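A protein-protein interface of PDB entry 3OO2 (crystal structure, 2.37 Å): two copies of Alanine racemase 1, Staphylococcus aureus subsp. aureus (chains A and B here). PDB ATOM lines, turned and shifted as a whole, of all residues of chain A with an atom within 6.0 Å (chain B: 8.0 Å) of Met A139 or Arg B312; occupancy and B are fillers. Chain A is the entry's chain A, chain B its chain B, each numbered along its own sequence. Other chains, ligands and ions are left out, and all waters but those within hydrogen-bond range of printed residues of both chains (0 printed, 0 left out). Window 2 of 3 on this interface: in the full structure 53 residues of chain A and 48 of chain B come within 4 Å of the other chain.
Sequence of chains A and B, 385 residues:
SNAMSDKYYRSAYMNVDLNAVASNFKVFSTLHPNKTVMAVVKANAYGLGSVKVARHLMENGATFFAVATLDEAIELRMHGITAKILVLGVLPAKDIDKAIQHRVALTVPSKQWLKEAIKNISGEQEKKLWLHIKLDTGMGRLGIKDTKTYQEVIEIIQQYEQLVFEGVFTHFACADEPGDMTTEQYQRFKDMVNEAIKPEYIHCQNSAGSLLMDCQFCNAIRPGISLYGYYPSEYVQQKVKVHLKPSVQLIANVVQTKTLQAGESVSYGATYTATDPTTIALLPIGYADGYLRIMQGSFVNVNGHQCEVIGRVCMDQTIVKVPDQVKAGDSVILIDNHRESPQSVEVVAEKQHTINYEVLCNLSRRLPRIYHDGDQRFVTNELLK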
ATOM      1  N   ASP A 136       7.833  27.986 -23.200  1.00  0.00           N
ATOM      2  CA  ASP A 136       9.281  27.963 -23.096  1.00  0.00           C
ATOM      3  C   ASP A 136       9.636  29.033 -22.089  1.00  0.00           C
ATOM      4  O   ASP A 136       9.388  30.227 -22.325  1.00  0.00           O
ATOM      5  CB  ASP A 136       9.890  28.300 -24.452  1.00  0.00           C
ATOM      6  CG  ASP A 136      11.391  28.532 -24.398  1.00  0.00           C
ATOM      7  OD1 ASP A 136      11.971  28.524 -23.286  1.00  0.00           O
ATOM      8  OD2 ASP A 136      11.985  28.763 -25.490  1.00  0.00           O
ATOM      9  N   THR A 137      10.225  28.612 -20.974  1.00  0.00           N
ATOM     10  CA  THR A 137      10.606  29.529 -19.903  1.00  0.00           C
ATOM     11  C   THR A 137      12.121  29.570 -19.602  1.00  0.00           C
ATOM     12  O   THR A 137      12.587  30.489 -18.928  1.00  0.00           O
ATOM     13  CB  THR A 137       9.853  29.160 -18.607  1.00  0.00           C
ATOM     14  OG1 THR A 137      10.179  27.818 -18.236  1.00  0.00           O
ATOM     15  CG2 THR A 137       8.323  29.267 -18.805  1.00  0.00           C
ATOM     16  N   GLY A 138      12.890  28.595 -20.089  1.00  0.00           N
ATOM     17  CA  GLY A 138      14.339  28.554 -19.817  1.00  0.00           C
ATOM     18  C   GLY A 138      15.161  28.099 -21.004  1.00  0.00           C
ATOM     19  O   GLY A 138      15.156  28.755 -22.045  1.00  0.00           O
ATOM     20  N   MET A 139      15.923  27.018 -20.848  1.00  0.00           N
ATOM     21  CA  MET A 139      16.654  26.479 -21.996  1.00  0.00           C
ATOM     22  C   MET A 139      15.567  26.243 -22.982  1.00  0.00           C
ATOM     23  O   MET A 139      14.946  25.190 -22.989  1.00  0.00           O
ATOM     24  CB  MET A 139      17.337  25.136 -21.721  1.00  0.00           C
ATOM     25  CG  MET A 139      18.607  25.188 -20.913  1.00  0.00           C
ATOM     26  SD  MET A 139      19.324  23.548 -21.007  1.00  0.00           S
ATOM     27  CE  MET A 139      20.819  23.766 -20.020  1.00  0.00           C
ATOM     28  N   GLY A 140      15.315  27.251 -23.791  1.00  0.00           N
ATOM     29  CA  GLY A 140      14.264  27.188 -24.751  1.00  0.00           C
ATOM     30  C   GLY A 140      14.496  26.189 -25.838  1.00  0.00           C
ATOM     31  O   GLY A 140      15.477  26.273 -26.582  1.00  0.00           O
ATOM     32  N   ARG A 141      13.613  25.203 -25.878  1.00  0.00           N
ATOM     33  CA  ARG A 141      13.593  24.233 -26.949  1.00  0.00           C
ATOM     34  C   ARG A 141      12.240  24.371 -27.652  1.00  0.00           C
ATOM     35  O   ARG A 141      12.105  25.106 -28.617  1.00  0.00           O
ATOM     36  CB  ARG A 141      13.786  22.808 -26.444  1.00  0.00           C
ATOM     37  CG  ARG A 141      15.157  22.533 -25.896  1.00  0.00           C
ATOM     38  CD  ARG A 141      15.358  21.053 -25.728  1.00  0.00           C
ATOM     39  NE  ARG A 141      16.638  20.755 -25.102  1.00  0.00           N
ATOM     40  CZ  ARG A 141      17.191  19.551 -25.070  1.00  0.00           C
ATOM     41  NH1 ARG A 141      16.597  18.532 -25.677  1.00  0.00           N
ATOM     42  NH2 ARG A 141      18.356  19.381 -24.474  1.00  0.00           N
ATOM     43  N   LEU A 142      11.245  23.672 -27.137  1.00  0.00           N
ATOM     44  CA  LEU A 142       9.929  23.668 -27.728  1.00  0.00           C
ATOM     45  C   LEU A 142       9.030  24.533 -26.867  1.00  0.00           C
ATOM     46  O   LEU A 142       9.238  24.643 -25.651  1.00  0.00           O
ATOM     47  CB  LEU A 142       9.415  22.225 -27.725  1.00  0.00           C
ATOM     48  CG  LEU A 142       8.408  21.801 -28.791  1.00  0.00           C
ATOM     49  CD1 LEU A 142       8.988  22.071 -30.152  1.00  0.00           C
ATOM     50  CD2 LEU A 142       8.059  20.325 -28.639  1.00  0.00           C
ATOM     51  N   PHE A 172      11.189  21.948 -16.897  1.00  0.00           N
ATOM     52  CA  PHE A 172      12.418  22.492 -16.357  1.00  0.00           C
ATOM     53  C   PHE A 172      13.578  21.753 -16.984  1.00  0.00           C
ATOM     54  O   PHE A 172      13.505  20.552 -17.238  1.00  0.00           O
ATOM     55  CB  PHE A 172      12.472  22.379 -14.825  1.00  0.00           C
ATOM     56  CG  PHE A 172      11.380  23.166 -14.110  1.00  0.00           C
ATOM     57  CD1 PHE A 172      11.114  24.489 -14.450  1.00  0.00           C
ATOM     58  CD2 PHE A 172      10.673  22.598 -13.050  1.00  0.00           C
ATOM     59  CE1 PHE A 172      10.136  25.198 -13.788  1.00  0.00           C
ATOM     60  CE2 PHE A 172       9.698  23.322 -12.374  1.00  0.00           C
ATOM     61  CZ  PHE A 172       9.437  24.609 -12.730  1.00  0.00           C
ATOM     62  N   ALA A 173      14.646  22.485 -17.238  1.00  0.00           N
ATOM     63  CA  ALA A 173      15.828  21.927 -17.866  1.00  0.00           C
ATOM     64  C   ALA A 173      16.942  21.436 -16.912  1.00  0.00           C
ATOM     65  O   ALA A 173      17.725  20.579 -17.294  1.00  0.00           O
ATOM     66  CB  ALA A 173      16.411  22.969 -18.863  1.00  0.00           C
ATOM     67  N   CYS A 174      17.015  21.947 -15.693  1.00  0.00           N
ATOM     68  CA  CYS A 174      18.067  21.480 -14.792  1.00  0.00           C
ATOM     69  C   CYS A 174      17.616  21.340 -13.341  1.00  0.00           C
ATOM     70  O   CYS A 174      18.375  21.621 -12.411  1.00  0.00           O
ATOM     71  CB  CYS A 174      19.305  22.372 -14.914  1.00  0.00           C
ATOM     72  SG  CYS A 174      20.130  22.242 -16.535  1.00  0.00           S
ATOM     73  N   MET A 181      18.102  28.218 -12.123  1.00  0.00           N
ATOM     74  CA  MET A 181      17.364  28.180 -13.381  1.00  0.00           C
ATOM     75  C   MET A 181      15.931  27.782 -13.102  1.00  0.00           C
ATOM     76  O   MET A 181      14.993  28.519 -13.451  1.00  0.00           O
ATOM     77  CB  MET A 181      17.984  27.187 -14.370  1.00  0.00           C
ATOM     78  CG  MET A 181      19.356  27.593 -14.913  1.00  0.00           C
ATOM     79  SD  MET A 181      20.058  26.360 -16.040  1.00  0.00           S
ATOM     80  CE  MET A 181      18.776  26.295 -17.306  1.00  0.00           C
ATOM     81  N   GLN A 185      12.611  29.747 -14.082  1.00  0.00           N
ATOM     82  CA  GLN A 185      11.598  29.307 -15.025  1.00  0.00           C
ATOM     83  C   GLN A 185      10.216  29.365 -14.377  1.00  0.00           C
ATOM     84  O   GLN A 185       9.234  29.820 -15.002  1.00  0.00           O
ATOM     85  CB  GLN A 185      11.877  27.894 -15.512  1.00  0.00           C
ATOM     86  CG  GLN A 185      13.184  27.764 -16.278  1.00  0.00           C
ATOM     87  CD  GLN A 185      13.313  26.430 -16.996  1.00  0.00           C
ATOM     88  OE1 GLN A 185      14.177  25.633 -16.655  1.00  0.00           O
ATOM     89  NE2 GLN A 185      12.410  26.157 -17.959  1.00  0.00           N
ATOM     90  N   LYS B 258      14.253  27.130 -34.059  1.00  0.00           N
ATOM     91  CA  LYS B 258      14.372  28.240 -33.164  1.00  0.00           C
ATOM     92  C   LYS B 258      15.732  28.862 -33.392  1.00  0.00           C
ATOM     93  O   LYS B 258      16.716  28.194 -33.655  1.00  0.00           O
ATOM     94  CB  LYS B 258      14.182  27.818 -31.701  1.00  0.00           C
ATOM     95  CG  LYS B 258      14.363  28.985 -30.695  1.00  0.00           C
ATOM     96  CD  LYS B 258      13.319  30.121 -30.910  1.00  0.00           C
ATOM     97  CE  LYS B 258      13.643  31.387 -30.093  1.00  0.00           C
ATOM     98  NZ  LYS B 258      13.844  31.106 -28.634  1.00  0.00           N
ATOM     99  N   LEU B 260      18.790  31.099 -31.999  1.00  0.00           N
ATOM    100  CA  LEU B 260      19.457  31.496 -30.778  1.00  0.00           C
ATOM    101  C   LEU B 260      20.338  32.703 -31.030  1.00  0.00           C
ATOM    102  O   LEU B 260      20.589  33.070 -32.174  1.00  0.00           O
ATOM    103  CB  LEU B 260      20.333  30.364 -30.265  1.00  0.00           C
ATOM    104  CG  LEU B 260      19.651  29.120 -29.713  1.00  0.00           C
ATOM    105  CD1 LEU B 260      20.724  28.106 -29.293  1.00  0.00           C
ATOM    106  CD2 LEU B 260      18.783  29.504 -28.540  1.00  0.00           C
ATOM    107  N   ILE B 280      18.582  26.371 -34.436  1.00  0.00           N
ATOM    108  CA  ILE B 280      18.541  24.968 -34.055  1.00  0.00           C
ATOM    109  C   ILE B 280      17.244  24.332 -34.545  1.00  0.00           C
ATOM    110  O   ILE B 280      16.230  24.986 -34.684  1.00  0.00           O
ATOM    111  CB  ILE B 280      18.695  24.767 -32.549  1.00  0.00           C
ATOM    112  CG1 ILE B 280      17.434  25.233 -31.801  1.00  0.00           C
ATOM    113  CG2 ILE B 280      19.977  25.461 -32.057  1.00  0.00           C
ATOM    114  CD1 ILE B 280      17.622  25.269 -30.300  1.00  0.00           C
ATOM    115  N   LEU B 282      14.604  20.961 -34.035  1.00  0.00           N
ATOM    116  CA  LEU B 282      14.214  19.956 -33.095  1.00  0.00           C
ATOM    117  C   LEU B 282      13.613  18.761 -33.847  1.00  0.00           C
ATOM    118  O   LEU B 282      12.673  18.913 -34.612  1.00  0.00           O
ATOM    119  CB  LEU B 282      13.266  20.556 -32.047  1.00  0.00           C
ATOM    120  CG  LEU B 282      13.879  21.724 -31.209  1.00  0.00           C
ATOM    121  CD1 LEU B 282      14.270  22.929 -32.066  1.00  0.00           C
ATOM    122  CD2 LEU B 282      12.951  22.235 -30.090  1.00  0.00           C
ATOM    123  N   TYR B 287      16.997   8.784 -27.705  1.00  0.00           N
ATOM    124  CA  TYR B 287      17.552   7.491 -27.242  1.00  0.00           C
ATOM    125  C   TYR B 287      16.525   6.378 -26.980  1.00  0.00           C
ATOM    126  O   TYR B 287      16.883   5.223 -27.056  1.00  0.00           O
ATOM    127  CB  TYR B 287      18.546   7.640 -26.091  1.00  0.00           C
ATOM    128  CG  TYR B 287      18.017   8.227 -24.814  1.00  0.00           C
ATOM    129  CD1 TYR B 287      18.194   9.566 -24.513  1.00  0.00           C
ATOM    130  CD2 TYR B 287      17.393   7.431 -23.882  1.00  0.00           C
ATOM    131  CE1 TYR B 287      17.752  10.088 -23.338  1.00  0.00           C
ATOM    132  CE2 TYR B 287      16.939   7.944 -22.688  1.00  0.00           C
ATOM    133  CZ  TYR B 287      17.115   9.272 -22.420  1.00  0.00           C
ATOM    134  OH  TYR B 287      16.635   9.772 -21.247  1.00  0.00           O
ATOM    135  N   LEU B 292      21.230   6.802 -29.519  1.00  0.00           N
ATOM    136  CA  LEU B 292      21.823   6.981 -28.182  1.00  0.00           C
ATOM    137  C   LEU B 292      22.378   8.348 -27.825  1.00  0.00           C
ATOM    138  O   LEU B 292      22.730   9.142 -28.689  1.00  0.00           O
ATOM    139  CB  LEU B 292      22.900   5.926 -27.943  1.00  0.00           C
ATOM    140  CG  LEU B 292      22.428   4.482 -28.161  1.00  0.00           C
ATOM    141  CD1 LEU B 292      23.434   3.551 -27.566  1.00  0.00           C
ATOM    142  CD2 LEU B 292      21.044   4.191 -27.523  1.00  0.00           C
ATOM    143  N   ARG B 293      22.472   8.597 -26.519  1.00  0.00           N
ATOM    144  CA  ARG B 293      22.953   9.875 -25.980  1.00  0.00           C
ATOM    145  C   ARG B 293      24.328  10.266 -26.458  1.00  0.00           C
ATOM    146  O   ARG B 293      24.627  11.449 -26.572  1.00  0.00           O
ATOM    147  CB  ARG B 293      22.952   9.880 -24.444  1.00  0.00           C
ATOM    148  CG  ARG B 293      21.568   9.841 -23.867  1.00  0.00           C
ATOM    149  CD  ARG B 293      21.559   9.759 -22.356  1.00  0.00           C
ATOM    150  NE  ARG B 293      21.940  11.008 -21.717  1.00  0.00           N
ATOM    151  CZ  ARG B 293      23.068  11.211 -21.072  1.00  0.00           C
ATOM    152  NH1 ARG B 293      23.968  10.247 -20.949  1.00  0.00           N
ATOM    153  NH2 ARG B 293      23.282  12.382 -20.529  1.00  0.00           N
ATOM    154  N   ILE B 294      25.152   9.265 -26.724  1.00  0.00           N
ATOM    155  CA  ILE B 294      26.514   9.487 -27.159  1.00  0.00           C
ATOM    156  C   ILE B 294      26.561  10.040 -28.601  1.00  0.00           C
ATOM    157  O   ILE B 294      27.633  10.451 -29.075  1.00  0.00           O
ATOM    158  CB  ILE B 294      27.347   8.164 -27.029  1.00  0.00           C
ATOM    159  CG1 ILE B 294      28.861   8.441 -27.107  1.00  0.00           C
ATOM    160  CG2 ILE B 294      26.878   7.144 -28.081  1.00  0.00           C
ATOM    161  CD1 ILE B 294      29.752   7.164 -26.889  1.00  0.00           C
ATOM    162  N   MET B 295      25.409  10.085 -29.287  1.00  0.00           N
ATOM    163  CA  MET B 295      25.388  10.609 -30.638  1.00  0.00           C
ATOM    164  C   MET B 295      25.604  12.133 -30.622  1.00  0.00           C
ATOM    165  O   MET B 295      25.824  12.731 -31.661  1.00  0.00           O
ATOM    166  CB  MET B 295      24.092  10.246 -31.395  1.00  0.00           C
ATOM    167  CG  MET B 295      23.881   8.778 -31.680  1.00  0.00           C
ATOM    168  SD  MET B 295      25.243   7.961 -32.487  1.00  0.00           S
ATOM    169  CE  MET B 295      25.414   8.890 -34.000  1.00  0.00           C
ATOM    170  N   GLN B 296      25.509  12.764 -29.459  1.00  0.00           N
ATOM    171  CA  GLN B 296      25.799  14.185 -29.375  1.00  0.00           C
ATOM    172  C   GLN B 296      27.198  14.398 -29.940  1.00  0.00           C
ATOM    173  O   GLN B 296      28.116  13.696 -29.560  1.00  0.00           O
ATOM    174  CB  GLN B 296      25.761  14.660 -27.926  1.00  0.00           C
ATOM    175  CG  GLN B 296      26.036  16.161 -27.742  1.00  0.00           C
ATOM    176  CD  GLN B 296      26.093  16.540 -26.279  1.00  0.00           C
ATOM    177  OE1 GLN B 296      25.902  15.688 -25.413  1.00  0.00           O
ATOM    178  NE2 GLN B 296      26.346  17.810 -25.990  1.00  0.00           N
ATOM    179  N   VAL B 309      24.810  17.539 -34.157  1.00  0.00           N
ATOM    180  CA  VAL B 309      23.831  17.250 -33.131  1.00  0.00           C
ATOM    181  C   VAL B 309      24.378  17.891 -31.865  1.00  0.00           C
ATOM    182  O   VAL B 309      25.435  17.525 -31.432  1.00  0.00           O
ATOM    183  CB  VAL B 309      23.654  15.762 -32.937  1.00  0.00           C
ATOM    184  CG1 VAL B 309      22.795  15.474 -31.697  1.00  0.00           C
ATOM    185  CG2 VAL B 309      23.067  15.140 -34.204  1.00  0.00           C
ATOM    186  N   ILE B 310      23.672  18.890 -31.323  1.00  0.00           N
ATOM    187  CA  ILE B 310      24.114  19.623 -30.147  1.00  0.00           C
ATOM    188  C   ILE B 310      23.213  19.453 -28.965  1.00  0.00           C
ATOM    189  O   ILE B 310      22.044  19.059 -29.086  1.00  0.00           O
ATOM    190  CB  ILE B 310      24.296  21.174 -30.371  1.00  0.00           C
ATOM    191  CG1 ILE B 310      23.032  21.818 -30.963  1.00  0.00           C
ATOM    192  CG2 ILE B 310      25.506  21.449 -31.237  1.00  0.00           C
ATOM    193  CD1 ILE B 310      23.052  23.363 -30.930  1.00  0.00           C
ATOM    194  N   GLY B 311      23.783  19.793 -27.808  1.00  0.00           N
ATOM    195  CA  GLY B 311      23.116  19.645 -26.541  1.00  0.00           C
ATOM    196  C   GLY B 311      22.940  18.169 -26.257  1.00  0.00           C
ATOM    197  O   GLY B 311      23.433  17.306 -26.986  1.00  0.00           O
ATOM    198  N   ARG B 312      22.228  17.879 -25.189  1.00  0.00           N
ATOM    199  CA  ARG B 312      21.965  16.503 -24.822  1.00  0.00           C
ATOM    200  C   ARG B 312      20.908  15.916 -25.752  1.00  0.00           C
ATOM    201  O   ARG B 312      19.966  16.614 -26.132  1.00  0.00           O
ATOM    202  CB  ARG B 312      21.524  16.442 -23.336  1.00  0.00           C
ATOM    203  CG  ARG B 312      20.335  17.330 -22.986  1.00  0.00           C
ATOM    204  CD  ARG B 312      20.075  17.460 -21.451  1.00  0.00           C
ATOM    205  NE  ARG B 312      18.863  18.251 -21.134  1.00  0.00           N
ATOM    206  CZ  ARG B 312      18.836  19.567 -20.903  1.00  0.00           C
ATOM    207  NH1 ARG B 312      19.948  20.299 -20.937  1.00  0.00           N
ATOM    208  NH2 ARG B 312      17.681  20.166 -20.624  1.00  0.00           N
ATOM    209  N   VAL B 313      21.125  14.674 -26.199  1.00  0.00           N
ATOM    210  CA  VAL B 313      20.106  13.936 -26.959  1.00  0.00           C
ATOM    211  C   VAL B 313      19.133  13.471 -25.864  1.00  0.00           C
ATOM    212  O   VAL B 313      19.555  12.870 -24.902  1.00  0.00           O
ATOM    213  CB  VAL B 313      20.670  12.678 -27.686  1.00  0.00           C
ATOM    214  CG1 VAL B 313      19.538  11.782 -28.185  1.00  0.00           C
ATOM    215  CG2 VAL B 313      21.621  13.045 -28.815  1.00  0.00           C
ATOM    216  N   CYS B 314      17.848  13.786 -26.017  1.00  0.00           N
ATOM    217  CA  CYS B 314      16.821  13.417 -25.038  1.00  0.00           C
ATOM    218  C   CYS B 314      16.158  12.080 -25.376  1.00  0.00           C
ATOM    219  O   CYS B 314      16.457  11.469 -26.401  1.00  0.00           O
ATOM    220  CB  CYS B 314      15.752  14.513 -24.963  1.00  0.00           C
ATOM    221  SG  CYS B 314      16.364  16.105 -24.385  1.00  0.00           S
ATOM    222  N   MET B 315      15.260  11.626 -24.505  1.00  0.00           N
ATOM    223  CA  MET B 315      14.555  10.366 -24.725  1.00  0.00           C
ATOM    224  C   MET B 315      13.750  10.401 -26.018  1.00  0.00           C
ATOM    225  O   MET B 315      13.740   9.438 -26.775  1.00  0.00           O
ATOM    226  CB  MET B 315      13.623  10.060 -23.549  1.00  0.00           C
ATOM    227  CG  MET B 315      13.118   8.608 -23.538  1.00  0.00           C
ATOM    228  SD  MET B 315      12.041   8.186 -22.134  1.00  0.00           S
ATOM    229  CE  MET B 315      13.143   8.609 -20.804  1.00  0.00           C
ATOM    230  N   GLN B 317      13.641  13.623 -28.096  1.00  0.00           N
ATOM    231  CA  GLN B 317      14.064  14.663 -29.015  1.00  0.00           C
ATOM    232  C   GLN B 317      15.577  14.782 -29.159  1.00  0.00           C
ATOM    233  O   GLN B 317      16.341  14.499 -28.236  1.00  0.00           O
ATOM    234  CB  GLN B 317      13.582  16.033 -28.561  1.00  0.00           C
ATOM    235  CG  GLN B 317      12.081  16.201 -28.450  1.00  0.00           C
ATOM    236  CD  GLN B 317      11.703  17.636 -28.059  1.00  0.00           C
ATOM    237  OE1 GLN B 317      12.572  18.508 -27.900  1.00  0.00           O
ATOM    238  NE2 GLN B 317      10.409  17.882 -27.923  1.00  0.00           N
ATOM    239  N   THR B 318      15.970  15.289 -30.325  1.00  0.00           N
ATOM    240  CA  THR B 318      17.357  15.526 -30.678  1.00  0.00           C
ATOM    241  C   THR B 318      17.395  16.936 -31.250  1.00  0.00           C
ATOM    242  O   THR B 318      16.465  17.331 -31.950  1.00  0.00           O
ATOM    243  CB  THR B 318      17.838  14.501 -31.745  1.00  0.00           C
ATOM    244  OG1 THR B 318      17.663  13.185 -31.242  1.00  0.00           O
ATOM    245  CG2 THR B 318      19.301  14.696 -32.098  1.00  0.00           C
ATOM    246  N   ILE B 319      18.433  17.700 -30.916  1.00  0.00           N
ATOM    247  CA  ILE B 319      18.579  19.057 -31.418  1.00  0.00           C
ATOM    248  C   ILE B 319      19.784  19.159 -32.334  1.00  0.00           C
ATOM    249  O   ILE B 319      20.876  18.691 -31.987  1.00  0.00           O
ATOM    250  CB  ILE B 319      18.752  20.081 -30.277  1.00  0.00           C
ATOM    251  CG1 ILE B 319      17.533  20.088 -29.370  1.00  0.00           C
ATOM    252  CG2 ILE B 319      18.931  21.483 -30.841  1.00  0.00           C
ATOM    253  CD1 ILE B 319      17.573  21.211 -28.340  1.00  0.00           C
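NH1 of Arg B312 sits at hydrogen-bond distance from SD of Met A139 (3.3 Å). The guanidinium group (NH1) of Arg A141 sits at hydrogen-bond distance from the side-chain sulfur (SG) of Cys B314. NH2 of Arg B312 is in hydrogen-bond range of O of Ala A173 (3.4 Å).
The backbone NH (N) of Ala A173 lies within hydrogen-bond range of the side-chain amide oxygen (OE1) of Gln A185, 3.2 Å away. The backbone NH (N) of Tyr B287 lies within hydrogen-bond range of the backbone carbonyl oxygen (O) of Cys B314 (3.0 Å). O of Ile B319 lies within hydrogen-bond range of N of Ile B310, at 2.9 Å.
C of Arg A141 touches CD2 of Leu B282, at 3.3 Å. Arg A141 touches Arg B312 (NH2 to CG, 3.2 Å). NE of Arg A141 touches CD1 of Ile B319, at 3.4 Å. N of Leu A142 touches CD2 of Leu B282, 3.7 Å away. Gln B317 touches Leu A142.
Of chain B, only Arg B312 comes within 4 Å of Met A139. Arg B312 touches three residues of chain A. No residue of chain B comes within 4 Å of Gly A138. No residue of chain B comes within 4 Å of Gly A140. Printed residues of chain A within 4 Å of Gln B317: Leu A142. Of the printed residues of chain B, Ala A173 touches Arg B312 (3.4 Å). Of the printed residues of chain A, Ile B319 touches Arg A141. Ile B280 touches none of the printed residues of chain A. The nearest printed residue of chain A that does not touch Arg B312 is Cys A174 (4.8 Å).
Printed residues of chain B that touch a printed residue of chain A: Leu B282, Arg B312, Cys B314, Gln B317 and Ile B319. Hydrophobic or aromatic side chains of chain B that line the printed part of chain A: Leu B282 and Ile B319. Of the 12 printed residues of chain A, 4 touch a printed residue of chain B. Printed residues of chain A that touch a printed residue of chain B: Met A139, Arg A141, Leu A142 and Ala A173. Hydrophobic or aromatic side chains of chain A within 4 Å of the printed part of chain B: Met A139, Leu A142 and Ala A173. Among the printed residues, no Asp or Glu carboxylate lies within 4 Å of a Lys or Arg side-chain nitrogen of the other chain.
No position is printed for both chains. Of the 8 pairs that touch across the chains among the printed residues, none has its exchanged pair printed and touching as well.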
